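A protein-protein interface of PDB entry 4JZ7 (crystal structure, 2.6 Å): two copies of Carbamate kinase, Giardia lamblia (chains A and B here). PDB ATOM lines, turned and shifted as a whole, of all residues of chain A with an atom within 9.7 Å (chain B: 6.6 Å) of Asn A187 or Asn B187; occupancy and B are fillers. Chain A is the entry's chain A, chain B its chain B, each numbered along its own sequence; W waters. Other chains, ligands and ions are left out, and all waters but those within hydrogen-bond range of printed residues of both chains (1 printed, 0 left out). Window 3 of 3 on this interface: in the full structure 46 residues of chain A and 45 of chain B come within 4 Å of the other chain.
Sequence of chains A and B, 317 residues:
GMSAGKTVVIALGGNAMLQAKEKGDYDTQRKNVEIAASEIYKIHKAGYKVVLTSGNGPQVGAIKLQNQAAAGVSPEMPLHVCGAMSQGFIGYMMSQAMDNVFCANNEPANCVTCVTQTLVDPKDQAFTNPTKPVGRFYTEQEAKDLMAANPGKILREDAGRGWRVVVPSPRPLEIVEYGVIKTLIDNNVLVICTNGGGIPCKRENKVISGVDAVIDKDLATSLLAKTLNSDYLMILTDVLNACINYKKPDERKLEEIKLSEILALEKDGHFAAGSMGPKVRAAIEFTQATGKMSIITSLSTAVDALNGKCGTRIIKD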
ATOM      1  N   MET A   2     -36.507  30.719   3.075  1.00  0.00           N
ATOM      2  CA  MET A   2     -36.042  32.068   3.399  1.00  0.00           C
ATOM      3  C   MET A   2     -36.609  32.612   4.721  1.00  0.00           C
ATOM      4  O   MET A   2     -37.236  31.877   5.511  1.00  0.00           O
ATOM      5  CB  MET A   2     -36.351  33.027   2.223  1.00  0.00           C
ATOM      6  CG  MET A   2     -37.307  32.424   1.148  1.00  0.00           C
ATOM      7  SD  MET A   2     -37.962  33.572  -0.134  1.00  0.00           S
ATOM      8  CE  MET A   2     -39.331  32.601  -0.805  1.00  0.00           C
ATOM      9  N   SER A   3     -36.366  33.907   4.938  1.00  0.00           N
ATOM     10  CA  SER A   3     -36.605  34.573   6.213  1.00  0.00           C
ATOM     11  C   SER A   3     -38.079  34.633   6.617  1.00  0.00           C
ATOM     12  O   SER A   3     -38.396  34.589   7.803  1.00  0.00           O
ATOM     13  CB  SER A   3     -36.051  35.998   6.153  1.00  0.00           C
ATOM     14  OG  SER A   3     -34.694  36.026   5.730  1.00  0.00           O
ATOM     15  N   ALA A   4     -38.975  34.717   5.641  1.00  0.00           N
ATOM     16  CA  ALA A   4     -40.397  34.903   5.939  1.00  0.00           C
ATOM     17  C   ALA A   4     -41.045  33.699   6.608  1.00  0.00           C
ATOM     18  O   ALA A   4     -42.068  33.829   7.290  1.00  0.00           O
ATOM     19  CB  ALA A   4     -41.173  35.244   4.652  1.00  0.00           C
ATOM     20  N   GLY A   5     -40.432  32.529   6.416  1.00  0.00           N
ATOM     21  CA  GLY A   5     -41.047  31.261   6.729  1.00  0.00           C
ATOM     22  C   GLY A   5     -41.324  30.962   8.190  1.00  0.00           C
ATOM     23  O   GLY A   5     -40.545  31.340   9.086  1.00  0.00           O
ATOM     24  N   THR A   7     -41.742  28.238  11.334  1.00  0.00           N
ATOM     25  CA  THR A   7     -40.811  27.222  11.769  1.00  0.00           C
ATOM     26  C   THR A   7     -41.596  25.976  12.057  1.00  0.00           C
ATOM     27  O   THR A   7     -42.649  26.057  12.656  1.00  0.00           O
ATOM     28  CB  THR A   7     -40.092  27.609  13.054  1.00  0.00           C
ATOM     29  OG1 THR A   7     -39.226  28.722  12.814  1.00  0.00           O
ATOM     30  CG2 THR A   7     -39.266  26.441  13.560  1.00  0.00           C
ATOM     31  N   HIS A  44     -39.283  22.266   3.170  1.00  0.00           N
ATOM     32  CA  HIS A  44     -38.431  23.428   2.982  1.00  0.00           C
ATOM     33  C   HIS A  44     -38.746  24.211   1.692  1.00  0.00           C
ATOM     34  O   HIS A  44     -38.667  25.445   1.673  1.00  0.00           O
ATOM     35  CB  HIS A  44     -36.964  23.018   2.985  1.00  0.00           C
ATOM     36  CG  HIS A  44     -36.053  24.100   2.498  1.00  0.00           C
ATOM     37  ND1 HIS A  44     -35.508  25.046   3.337  1.00  0.00           N
ATOM     38  CD2 HIS A  44     -35.624  24.410   1.249  1.00  0.00           C
ATOM     39  CE1 HIS A  44     -34.763  25.876   2.628  1.00  0.00           C
ATOM     40  NE2 HIS A  44     -34.817  25.510   1.359  1.00  0.00           N
ATOM     41  N   LYS A  49     -39.406  26.910   7.569  1.00  0.00           N
ATOM     42  CA  LYS A  49     -38.129  26.826   8.264  1.00  0.00           C
ATOM     43  C   LYS A  49     -38.112  25.468   8.945  1.00  0.00           C
ATOM     44  O   LYS A  49     -39.088  25.125   9.615  1.00  0.00           O
ATOM     45  CB  LYS A  49     -38.050  27.929   9.308  1.00  0.00           C
ATOM     46  CG  LYS A  49     -36.922  28.957   9.094  1.00  0.00           C
ATOM     47  CD  LYS A  49     -37.441  30.373   8.933  1.00  0.00           C
ATOM     48  CE  LYS A  49     -36.480  31.397   9.523  1.00  0.00           C
ATOM     49  NZ  LYS A  49     -36.726  31.660  10.978  1.00  0.00           N
ATOM     50  N   VAL A  50     -37.037  24.687   8.788  1.00  0.00           N
ATOM     51  CA  VAL A  50     -37.056  23.320   9.319  1.00  0.00           C
ATOM     52  C   VAL A  50     -36.015  22.995  10.400  1.00  0.00           C
ATOM     53  O   VAL A  50     -34.825  23.310  10.274  1.00  0.00           O
ATOM     54  CB  VAL A  50     -36.934  22.267   8.211  1.00  0.00           C
ATOM     55  CG1 VAL A  50     -36.915  20.882   8.817  1.00  0.00           C
ATOM     56  CG2 VAL A  50     -38.091  22.394   7.243  1.00  0.00           C
ATOM     57  N   ASN A 110     -27.409  24.224   2.598  1.00  0.00           N
ATOM     58  CA  ASN A 110     -27.391  25.087   3.763  1.00  0.00           C
ATOM     59  C   ASN A 110     -27.989  24.450   5.016  1.00  0.00           C
ATOM     60  O   ASN A 110     -28.975  24.939   5.546  1.00  0.00           O
ATOM     61  CB  ASN A 110     -28.118  26.389   3.445  1.00  0.00           C
ATOM     62  CG  ASN A 110     -28.042  27.372   4.578  1.00  0.00           C
ATOM     63  OD1 ASN A 110     -26.963  27.610   5.129  1.00  0.00           O
ATOM     64  ND2 ASN A 110     -29.190  27.930   4.961  1.00  0.00           N
ATOM     65  N   CYS A 111     -27.395  23.346   5.461  1.00  0.00           N
ATOM     66  CA  CYS A 111     -27.877  22.640   6.638  1.00  0.00           C
ATOM     67  C   CYS A 111     -26.688  22.084   7.398  1.00  0.00           C
ATOM     68  O   CYS A 111     -25.592  22.005   6.860  1.00  0.00           O
ATOM     69  CB  CYS A 111     -28.824  21.504   6.242  1.00  0.00           C
ATOM     70  SG  CYS A 111     -27.965  19.983   5.853  1.00  0.00           S
ATOM     71  N   GLY A 179     -29.568  27.436  22.364  1.00  0.00           N
ATOM     72  CA  GLY A 179     -29.276  28.805  21.968  1.00  0.00           C
ATOM     73  C   GLY A 179     -28.670  28.883  20.570  1.00  0.00           C
ATOM     74  O   GLY A 179     -29.022  29.724  19.740  1.00  0.00           O
ATOM     75  N   VAL A 180     -27.731  27.987  20.306  1.00  0.00           N
ATOM     76  CA  VAL A 180     -27.092  27.894  19.008  1.00  0.00           C
ATOM     77  C   VAL A 180     -28.114  27.443  17.973  1.00  0.00           C
ATOM     78  O   VAL A 180     -28.081  27.851  16.809  1.00  0.00           O
ATOM     79  CB  VAL A 180     -25.976  26.853  19.086  1.00  0.00           C
ATOM     80  CG1 VAL A 180     -25.288  26.695  17.742  1.00  0.00           C
ATOM     81  CG2 VAL A 180     -24.987  27.230  20.208  1.00  0.00           C
ATOM     82  N   ILE A 181     -29.039  26.598  18.411  1.00  0.00           N
ATOM     83  CA  ILE A 181     -30.059  26.079  17.521  1.00  0.00           C
ATOM     84  C   ILE A 181     -30.974  27.228  17.069  1.00  0.00           C
ATOM     85  O   ILE A 181     -31.245  27.417  15.882  1.00  0.00           O
ATOM     86  CB  ILE A 181     -30.813  24.898  18.176  1.00  0.00           C
ATOM     87  CG1 ILE A 181     -29.825  23.749  18.427  1.00  0.00           C
ATOM     88  CG2 ILE A 181     -31.967  24.434  17.308  1.00  0.00           C
ATOM     89  CD1 ILE A 181     -30.428  22.462  18.970  1.00  0.00           C
ATOM     90  N   LYS A 182     -31.428  28.030  18.021  1.00  0.00           N
ATOM     91  CA  LYS A 182     -32.212  29.214  17.681  1.00  0.00           C
ATOM     92  C   LYS A 182     -31.462  30.163  16.723  1.00  0.00           C
ATOM     93  O   LYS A 182     -32.043  30.615  15.720  1.00  0.00           O
ATOM     94  CB  LYS A 182     -32.635  29.972  18.949  1.00  0.00           C
ATOM     95  CG  LYS A 182     -33.851  30.849  18.745  1.00  0.00           C
ATOM     96  CD  LYS A 182     -33.503  32.330  18.798  1.00  0.00           C
ATOM     97  CE  LYS A 182     -34.770  33.195  18.756  1.00  0.00           C
ATOM     98  NZ  LYS A 182     -35.634  32.909  17.554  1.00  0.00           N
ATOM     99  N   THR A 183     -30.206  30.487  17.058  1.00  0.00           N
ATOM    100  CA  THR A 183     -29.331  31.263  16.179  1.00  0.00           C
ATOM    101  C   THR A 183     -29.322  30.717  14.740  1.00  0.00           C
ATOM    102  O   THR A 183     -29.415  31.475  13.786  1.00  0.00           O
ATOM    103  CB  THR A 183     -27.871  31.220  16.675  1.00  0.00           C
ATOM    104  OG1 THR A 183     -27.763  31.844  17.966  1.00  0.00           O
ATOM    105  CG2 THR A 183     -26.925  31.900  15.658  1.00  0.00           C
ATOM    106  N   LEU A 184     -29.218  29.401  14.603  1.00  0.00           N
ATOM    107  CA  LEU A 184     -29.157  28.771  13.294  1.00  0.00           C
ATOM    108  C   LEU A 184     -30.460  28.894  12.523  1.00  0.00           C
ATOM    109  O   LEU A 184     -30.439  29.153  11.320  1.00  0.00           O
ATOM    110  CB  LEU A 184     -28.725  27.297  13.402  1.00  0.00           C
ATOM    111  CG  LEU A 184     -27.254  27.042  13.743  1.00  0.00           C
ATOM    112  CD1 LEU A 184     -27.072  25.644  14.269  1.00  0.00           C
ATOM    113  CD2 LEU A 184     -26.355  27.297  12.537  1.00  0.00           C
ATOM    114  N   ILE A 185     -31.602  28.680  13.180  1.00  0.00           N
ATOM    115  CA  ILE A 185     -32.864  28.905  12.450  1.00  0.00           C
ATOM    116  C   ILE A 185     -33.169  30.401  12.217  1.00  0.00           C
ATOM    117  O   ILE A 185     -33.848  30.748  11.274  1.00  0.00           O
ATOM    118  CB  ILE A 185     -34.123  28.226  13.104  1.00  0.00           C
ATOM    119  CG1 ILE A 185     -33.802  27.639  14.462  1.00  0.00           C
ATOM    120  CG2 ILE A 185     -34.680  27.108  12.224  1.00  0.00           C
ATOM    121  CD1 ILE A 185     -35.064  27.267  15.234  1.00  0.00           C
ATOM    122  N   ASP A 186     -32.666  31.274  13.082  1.00  0.00           N
ATOM    123  CA  ASP A 186     -32.842  32.697  12.852  1.00  0.00           C
ATOM    124  C   ASP A 186     -32.055  33.094  11.629  1.00  0.00           C
ATOM    125  O   ASP A 186     -32.264  34.176  11.078  1.00  0.00           O
ATOM    126  CB  ASP A 186     -32.395  33.509  14.057  1.00  0.00           C
ATOM    127  CG  ASP A 186     -33.297  33.299  15.252  1.00  0.00           C
ATOM    128  OD1 ASP A 186     -34.329  32.603  15.088  1.00  0.00           O
ATOM    129  OD2 ASP A 186     -32.982  33.836  16.345  1.00  0.00           O
ATOM    130  N   ASN A 187     -31.177  32.198  11.192  1.00  0.00           N
ATOM    131  CA  ASN A 187     -30.374  32.445  10.001  1.00  0.00           C
ATOM    132  C   ASN A 187     -30.788  31.523   8.882  1.00  0.00           C
ATOM    133  O   ASN A 187     -30.095  31.379   7.882  1.00  0.00           O
ATOM    134  CB  ASN A 187     -28.887  32.309  10.327  1.00  0.00           C
ATOM    135  CG  ASN A 187     -28.333  33.567  10.939  1.00  0.00           C
ATOM    136  OD1 ASN A 187     -27.736  34.380  10.237  1.00  0.00           O
ATOM    137  ND2 ASN A 187     -28.571  33.764  12.239  1.00  0.00           N
ATOM    138  N   ASN A 188     -31.927  30.881   9.083  1.00  0.00           N
ATOM    139  CA  ASN A 188     -32.540  30.096   8.033  1.00  0.00           C
ATOM    140  C   ASN A 188     -31.645  28.931   7.627  1.00  0.00           C
ATOM    141  O   ASN A 188     -31.657  28.510   6.474  1.00  0.00           O
ATOM    142  CB  ASN A 188     -32.843  31.001   6.836  1.00  0.00           C
ATOM    143  CG  ASN A 188     -33.156  32.444   7.261  1.00  0.00           C
ATOM    144  OD1 ASN A 188     -33.897  32.675   8.231  1.00  0.00           O
ATOM    145  ND2 ASN A 188     -32.562  33.419   6.557  1.00  0.00           N
ATOM    146  N   VAL A 189     -30.868  28.425   8.584  1.00  0.00           N
ATOM    147  CA  VAL A 189     -30.146  27.172   8.399  1.00  0.00           C
ATOM    148  C   VAL A 189     -31.072  25.993   8.708  1.00  0.00           C
ATOM    149  O   VAL A 189     -31.846  26.021   9.661  1.00  0.00           O
ATOM    150  CB  VAL A 189     -28.914  27.081   9.309  1.00  0.00           C
ATOM    151  CG1 VAL A 189     -28.133  25.794   8.995  1.00  0.00           C
ATOM    152  CG2 VAL A 189     -28.036  28.296   9.132  1.00  0.00           C
ATOM    153  N   LEU A 190     -30.998  24.948   7.896  1.00  0.00           N
ATOM    154  CA  LEU A 190     -31.793  23.758   8.156  1.00  0.00           C
ATOM    155  C   LEU A 190     -31.066  22.907   9.206  1.00  0.00           C
ATOM    156  O   LEU A 190     -30.092  22.219   8.899  1.00  0.00           O
ATOM    157  CB  LEU A 190     -32.012  22.981   6.854  1.00  0.00           C
ATOM    158  CG  LEU A 190     -33.329  22.200   6.814  1.00  0.00           C
ATOM    159  CD1 LEU A 190     -33.473  21.413   5.509  1.00  0.00           C
ATOM    160  CD2 LEU A 190     -33.402  21.281   8.018  1.00  0.00           C
ATOM    161  N   VAL A 191     -31.528  22.988  10.454  1.00  0.00           N
ATOM    162  CA  VAL A 191     -30.805  22.386  11.580  1.00  0.00           C
ATOM    163  C   VAL A 191     -31.189  20.941  11.838  1.00  0.00           C
ATOM    164  O   VAL A 191     -32.372  20.636  11.936  1.00  0.00           O
ATOM    165  CB  VAL A 191     -31.071  23.167  12.853  1.00  0.00           C
ATOM    166  CG1 VAL A 191     -30.689  22.353  14.074  1.00  0.00           C
ATOM    167  CG2 VAL A 191     -30.316  24.453  12.823  1.00  0.00           C
ATOM    168  N   LYS B  49     -12.575  35.379  18.795  1.00  0.00           N
ATOM    169  CA  LYS B  49     -13.507  34.371  18.290  1.00  0.00           C
ATOM    170  C   LYS B  49     -12.751  33.077  17.996  1.00  0.00           C
ATOM    171  O   LYS B  49     -11.694  33.117  17.384  1.00  0.00           O
ATOM    172  CB  LYS B  49     -14.136  34.862  16.992  1.00  0.00           C
ATOM    173  CG  LYS B  49     -15.073  36.061  17.137  1.00  0.00           C
ATOM    174  CD  LYS B  49     -15.827  36.283  15.827  1.00  0.00           C
ATOM    175  CE  LYS B  49     -16.774  37.468  15.912  1.00  0.00           C
ATOM    176  NZ  LYS B  49     -17.339  37.818  14.572  1.00  0.00           N
ATOM    177  N   ASN B 110     -22.131  28.945  25.245  1.00  0.00           N
ATOM    178  CA  ASN B 110     -22.418  29.283  23.867  1.00  0.00           C
ATOM    179  C   ASN B 110     -21.472  28.588  22.909  1.00  0.00           C
ATOM    180  O   ASN B 110     -20.676  29.236  22.217  1.00  0.00           O
ATOM    181  CB  ASN B 110     -22.342  30.784  23.660  1.00  0.00           C
ATOM    182  CG  ASN B 110     -23.048  31.208  22.409  1.00  0.00           C
ATOM    183  OD1 ASN B 110     -24.066  30.608  22.047  1.00  0.00           O
ATOM    184  ND2 ASN B 110     -22.506  32.209  21.711  1.00  0.00           N
ATOM    185  N   LYS B 182     -19.219  29.707   9.041  1.00  0.00           N
ATOM    186  CA  LYS B 182     -19.082  31.137   8.853  1.00  0.00           C
ATOM    187  C   LYS B 182     -20.187  31.888   9.586  1.00  0.00           C
ATOM    188  O   LYS B 182     -19.917  32.800  10.345  1.00  0.00           O
ATOM    189  CB  LYS B 182     -19.143  31.455   7.357  1.00  0.00           C
ATOM    190  CG  LYS B 182     -18.531  32.782   7.001  1.00  0.00           C
ATOM    191  CD  LYS B 182     -19.592  33.804   6.599  1.00  0.00           C
ATOM    192  CE  LYS B 182     -18.959  35.173   6.262  1.00  0.00           C
ATOM    193  NZ  LYS B 182     -18.057  35.675   7.370  1.00  0.00           N
ATOM    194  N   THR B 183     -21.426  31.498   9.338  1.00  0.00           N
ATOM    195  CA  THR B 183     -22.579  32.075  10.002  1.00  0.00           C
ATOM    196  C   THR B 183     -22.410  32.049  11.537  1.00  0.00           C
ATOM    197  O   THR B 183     -22.664  33.052  12.230  1.00  0.00           O
ATOM    198  CB  THR B 183     -23.860  31.278   9.599  1.00  0.00           C
ATOM    199  OG1 THR B 183     -24.292  31.688   8.298  1.00  0.00           O
ATOM    200  CG2 THR B 183     -24.998  31.496  10.584  1.00  0.00           C
ATOM    201  N   LEU B 184     -21.963  30.901  12.044  1.00  0.00           N
ATOM    202  CA  LEU B 184     -21.929  30.627  13.470  1.00  0.00           C
ATOM    203  C   LEU B 184     -20.916  31.483  14.193  1.00  0.00           C
ATOM    204  O   LEU B 184     -21.156  31.900  15.332  1.00  0.00           O
ATOM    205  CB  LEU B 184     -21.668  29.137  13.741  1.00  0.00           C
ATOM    206  CG  LEU B 184     -22.904  28.228  13.753  1.00  0.00           C
ATOM    207  CD1 LEU B 184     -22.586  26.853  13.208  1.00  0.00           C
ATOM    208  CD2 LEU B 184     -23.490  28.148  15.160  1.00  0.00           C
ATOM    209  N   ILE B 185     -19.778  31.741  13.544  1.00  0.00           N
ATOM    210  CA  ILE B 185     -18.832  32.687  14.133  1.00  0.00           C
ATOM    211  C   ILE B 185     -19.287  34.120  13.935  1.00  0.00           C
ATOM    212  O   ILE B 185     -19.001  34.981  14.766  1.00  0.00           O
ATOM    213  CB  ILE B 185     -17.372  32.527  13.628  1.00  0.00           C
ATOM    214  CG1 ILE B 185     -17.336  31.886  12.253  1.00  0.00           C
ATOM    215  CG2 ILE B 185     -16.561  31.660  14.580  1.00  0.00           C
ATOM    216  CD1 ILE B 185     -15.932  31.639  11.760  1.00  0.00           C
ATOM    217  N   ASP B 186     -19.994  34.397  12.845  1.00  0.00           N
ATOM    218  CA  ASP B 186     -20.477  35.766  12.678  1.00  0.00           C
ATOM    219  C   ASP B 186     -21.390  36.115  13.841  1.00  0.00           C
ATOM    220  O   ASP B 186     -21.549  37.283  14.167  1.00  0.00           O
ATOM    221  CB  ASP B 186     -21.145  36.007  11.328  1.00  0.00           C
ATOM    222  CG  ASP B 186     -20.127  36.280  10.222  1.00  0.00           C
ATOM    223  OD1 ASP B 186     -18.949  36.588  10.566  1.00  0.00           O
ATOM    224  OD2 ASP B 186     -20.494  36.188   9.017  1.00  0.00           O
ATOM    225  N   ASN B 187     -21.948  35.082  14.476  1.00  0.00           N
ATOM    226  CA  ASN B 187     -22.769  35.257  15.674  1.00  0.00           C
ATOM    227  C   ASN B 187     -22.038  34.961  16.982  1.00  0.00           C
ATOM    228  O   ASN B 187     -22.658  34.845  18.046  1.00  0.00           O
ATOM    229  CB  ASN B 187     -24.068  34.459  15.574  1.00  0.00           C
ATOM    230  CG  ASN B 187     -25.042  35.086  14.611  1.00  0.00           C
ATOM    231  OD1 ASN B 187     -25.894  35.889  15.004  1.00  0.00           O
ATOM    232  ND2 ASN B 187     -24.910  34.749  13.337  1.00  0.00           N
ATOM    233  N   ASN B 188     -20.718  34.807  16.897  1.00  0.00           N
ATOM    234  CA  ASN B 188     -19.909  34.777  18.098  1.00  0.00           C
ATOM    235  C   ASN B 188     -20.103  33.467  18.846  1.00  0.00           C
ATOM    236  O   ASN B 188     -19.800  33.349  20.030  1.00  0.00           O
ATOM    237  CB  ASN B 188     -20.260  35.973  18.994  1.00  0.00           C
ATOM    238  CG  ASN B 188     -20.471  37.263  18.186  1.00  0.00           C
ATOM    239  OD1 ASN B 188     -19.660  37.602  17.322  1.00  0.00           O
ATOM    240  ND2 ASN B 188     -21.576  37.966  18.445  1.00  0.00           N
ATOM    241  N   VAL B 189     -20.602  32.470  18.132  1.00  0.00           N
ATOM    242  CA  VAL B 189     -20.688  31.132  18.689  1.00  0.00           C
ATOM    243  C   VAL B 189     -19.313  30.442  18.639  1.00  0.00           C
ATOM    244  O   VAL B 189     -18.556  30.579  17.678  1.00  0.00           O
ATOM    245  CB  VAL B 189     -21.733  30.282  17.953  1.00  0.00           C
ATOM    246  CG1 VAL B 189     -21.568  28.828  18.333  1.00  0.00           C
ATOM    247  CG2 VAL B 189     -23.143  30.765  18.277  1.00  0.00           C
ATOM    248  N   LEU B 190     -18.989  29.713  19.701  1.00  0.00           N
ATOM    249  CA  LEU B 190     -17.725  28.991  19.763  1.00  0.00           C
ATOM    250  C   LEU B 190     -17.900  27.607  19.102  1.00  0.00           C
ATOM    251  O   LEU B 190     -18.490  26.685  19.674  1.00  0.00           O
ATOM    252  CB  LEU B 190     -17.222  28.887  21.202  1.00  0.00           C
ATOM    253  CG  LEU B 190     -15.699  28.796  21.322  1.00  0.00           C
ATOM    254  CD1 LEU B 190     -15.238  28.502  22.761  1.00  0.00           C
ATOM    255  CD2 LEU B 190     -15.174  27.719  20.379  1.00  0.00           C
HETATM  256  O   HOH W   1     -26.008  30.316   6.700  1.00  0.00           O
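OG1 of Thr A183 sits at hydrogen-bond distance from O of Gly A179 (3.0 Å).
The backbone NH (N) of Val A189 is in hydrogen-bond range of the backbone carbonyl oxygen (O) of Leu A184 (2.9 Å).
ND2 of Asn A187 is in hydrogen-bond range of O of Thr A183, 2.9 Å away.
O of Thr B183 is in hydrogen-bond range of ND2 of Asn B187 (3.0 Å).
N of Leu B190 lies within hydrogen-bond range of O of Asn B110 (3.1 Å).
The backbone carbonyl oxygen (O) of Leu B184 is in hydrogen-bond range of the backbone NH (N) of Val B189 (2.9 Å).
Among the printed residues, merely in contact across the chains: Val A180 with Leu B184, Leu A184 with Leu B184, Thr A183 with Asn B187, Asn A187 with Thr B183, Asn A187 with Asn B187 and Val A180 with Asn B110.
Gly A5 touches none of the printed residues of chain B.
Of the printed residues of chain B, Val A180 touches Asn B110 and Leu B184.
Printed residues of chain B within 4 Å of Thr A183: Asn B187 (3.8 Å).
Of chain B, only Thr B183 (3.9 Å) and Asn B187 (3.9 Å) come within 4 Å of Asn A187.
Printed residues of chain A within 4 Å of Asn B110: Val A180.
Of the printed residues of chain A, Thr B183 touches Asn A187 (3.9 Å).
Of chain A, only Thr A183 (3.8 Å) and Asn A187 (3.9 Å) come within 4 Å of Asn B187.
No residue of chain A comes within 4 Å of Asn B188.
The nearest printed residue of chain A that does not touch Thr B183 is Val A189 (4.6 Å).
Of the 23 printed residues of chain A, 4 touch a printed residue of chain B.
Printed residues of chain A that touch a printed residue of chain B: Val A180, Thr A183, Leu A184 and Asn A187.
Of the 11 printed residues of chain B, 4 touch a printed residue of chain A.
Printed residues of chain B that touch a printed residue of chain A: Asn B110, Thr B183, Leu B184 and Asn B187.
Hydrophobic or aromatic side chains of chain B within 4 Å of the printed part of chain A: Leu B184.
Along chain B the printed residues that touch a printed residue of chain A span positions 110 to 187.
Among the printed residues, 6 pairs touch across the chains.
Among the printed residues, no Asp or Glu carboxylate lies within 4 Å of a Lys or Arg side-chain nitrogen of the other chain.
Thr A183 touches Asn B187, and with the chains exchanged Asn A187 touches Thr B183.
Leu A184 touches its own counterpart, Leu B184.
Asn B187 touches its own counterpart, Asn A187.
Positions printed for both chains: 49, 110, 182, 183, 184, 185, 186, 187, 188, 189 and 190.
Of the 6 pairs that touch across the chains among the printed residues, 4 have their exchanged pair printed and touching as well.
Water W1 lies within hydrogen-bond range of the side-chain hydroxyl (OG1) of Thr B183 and the side-chain amide oxygen (OD1) of Asn A110.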
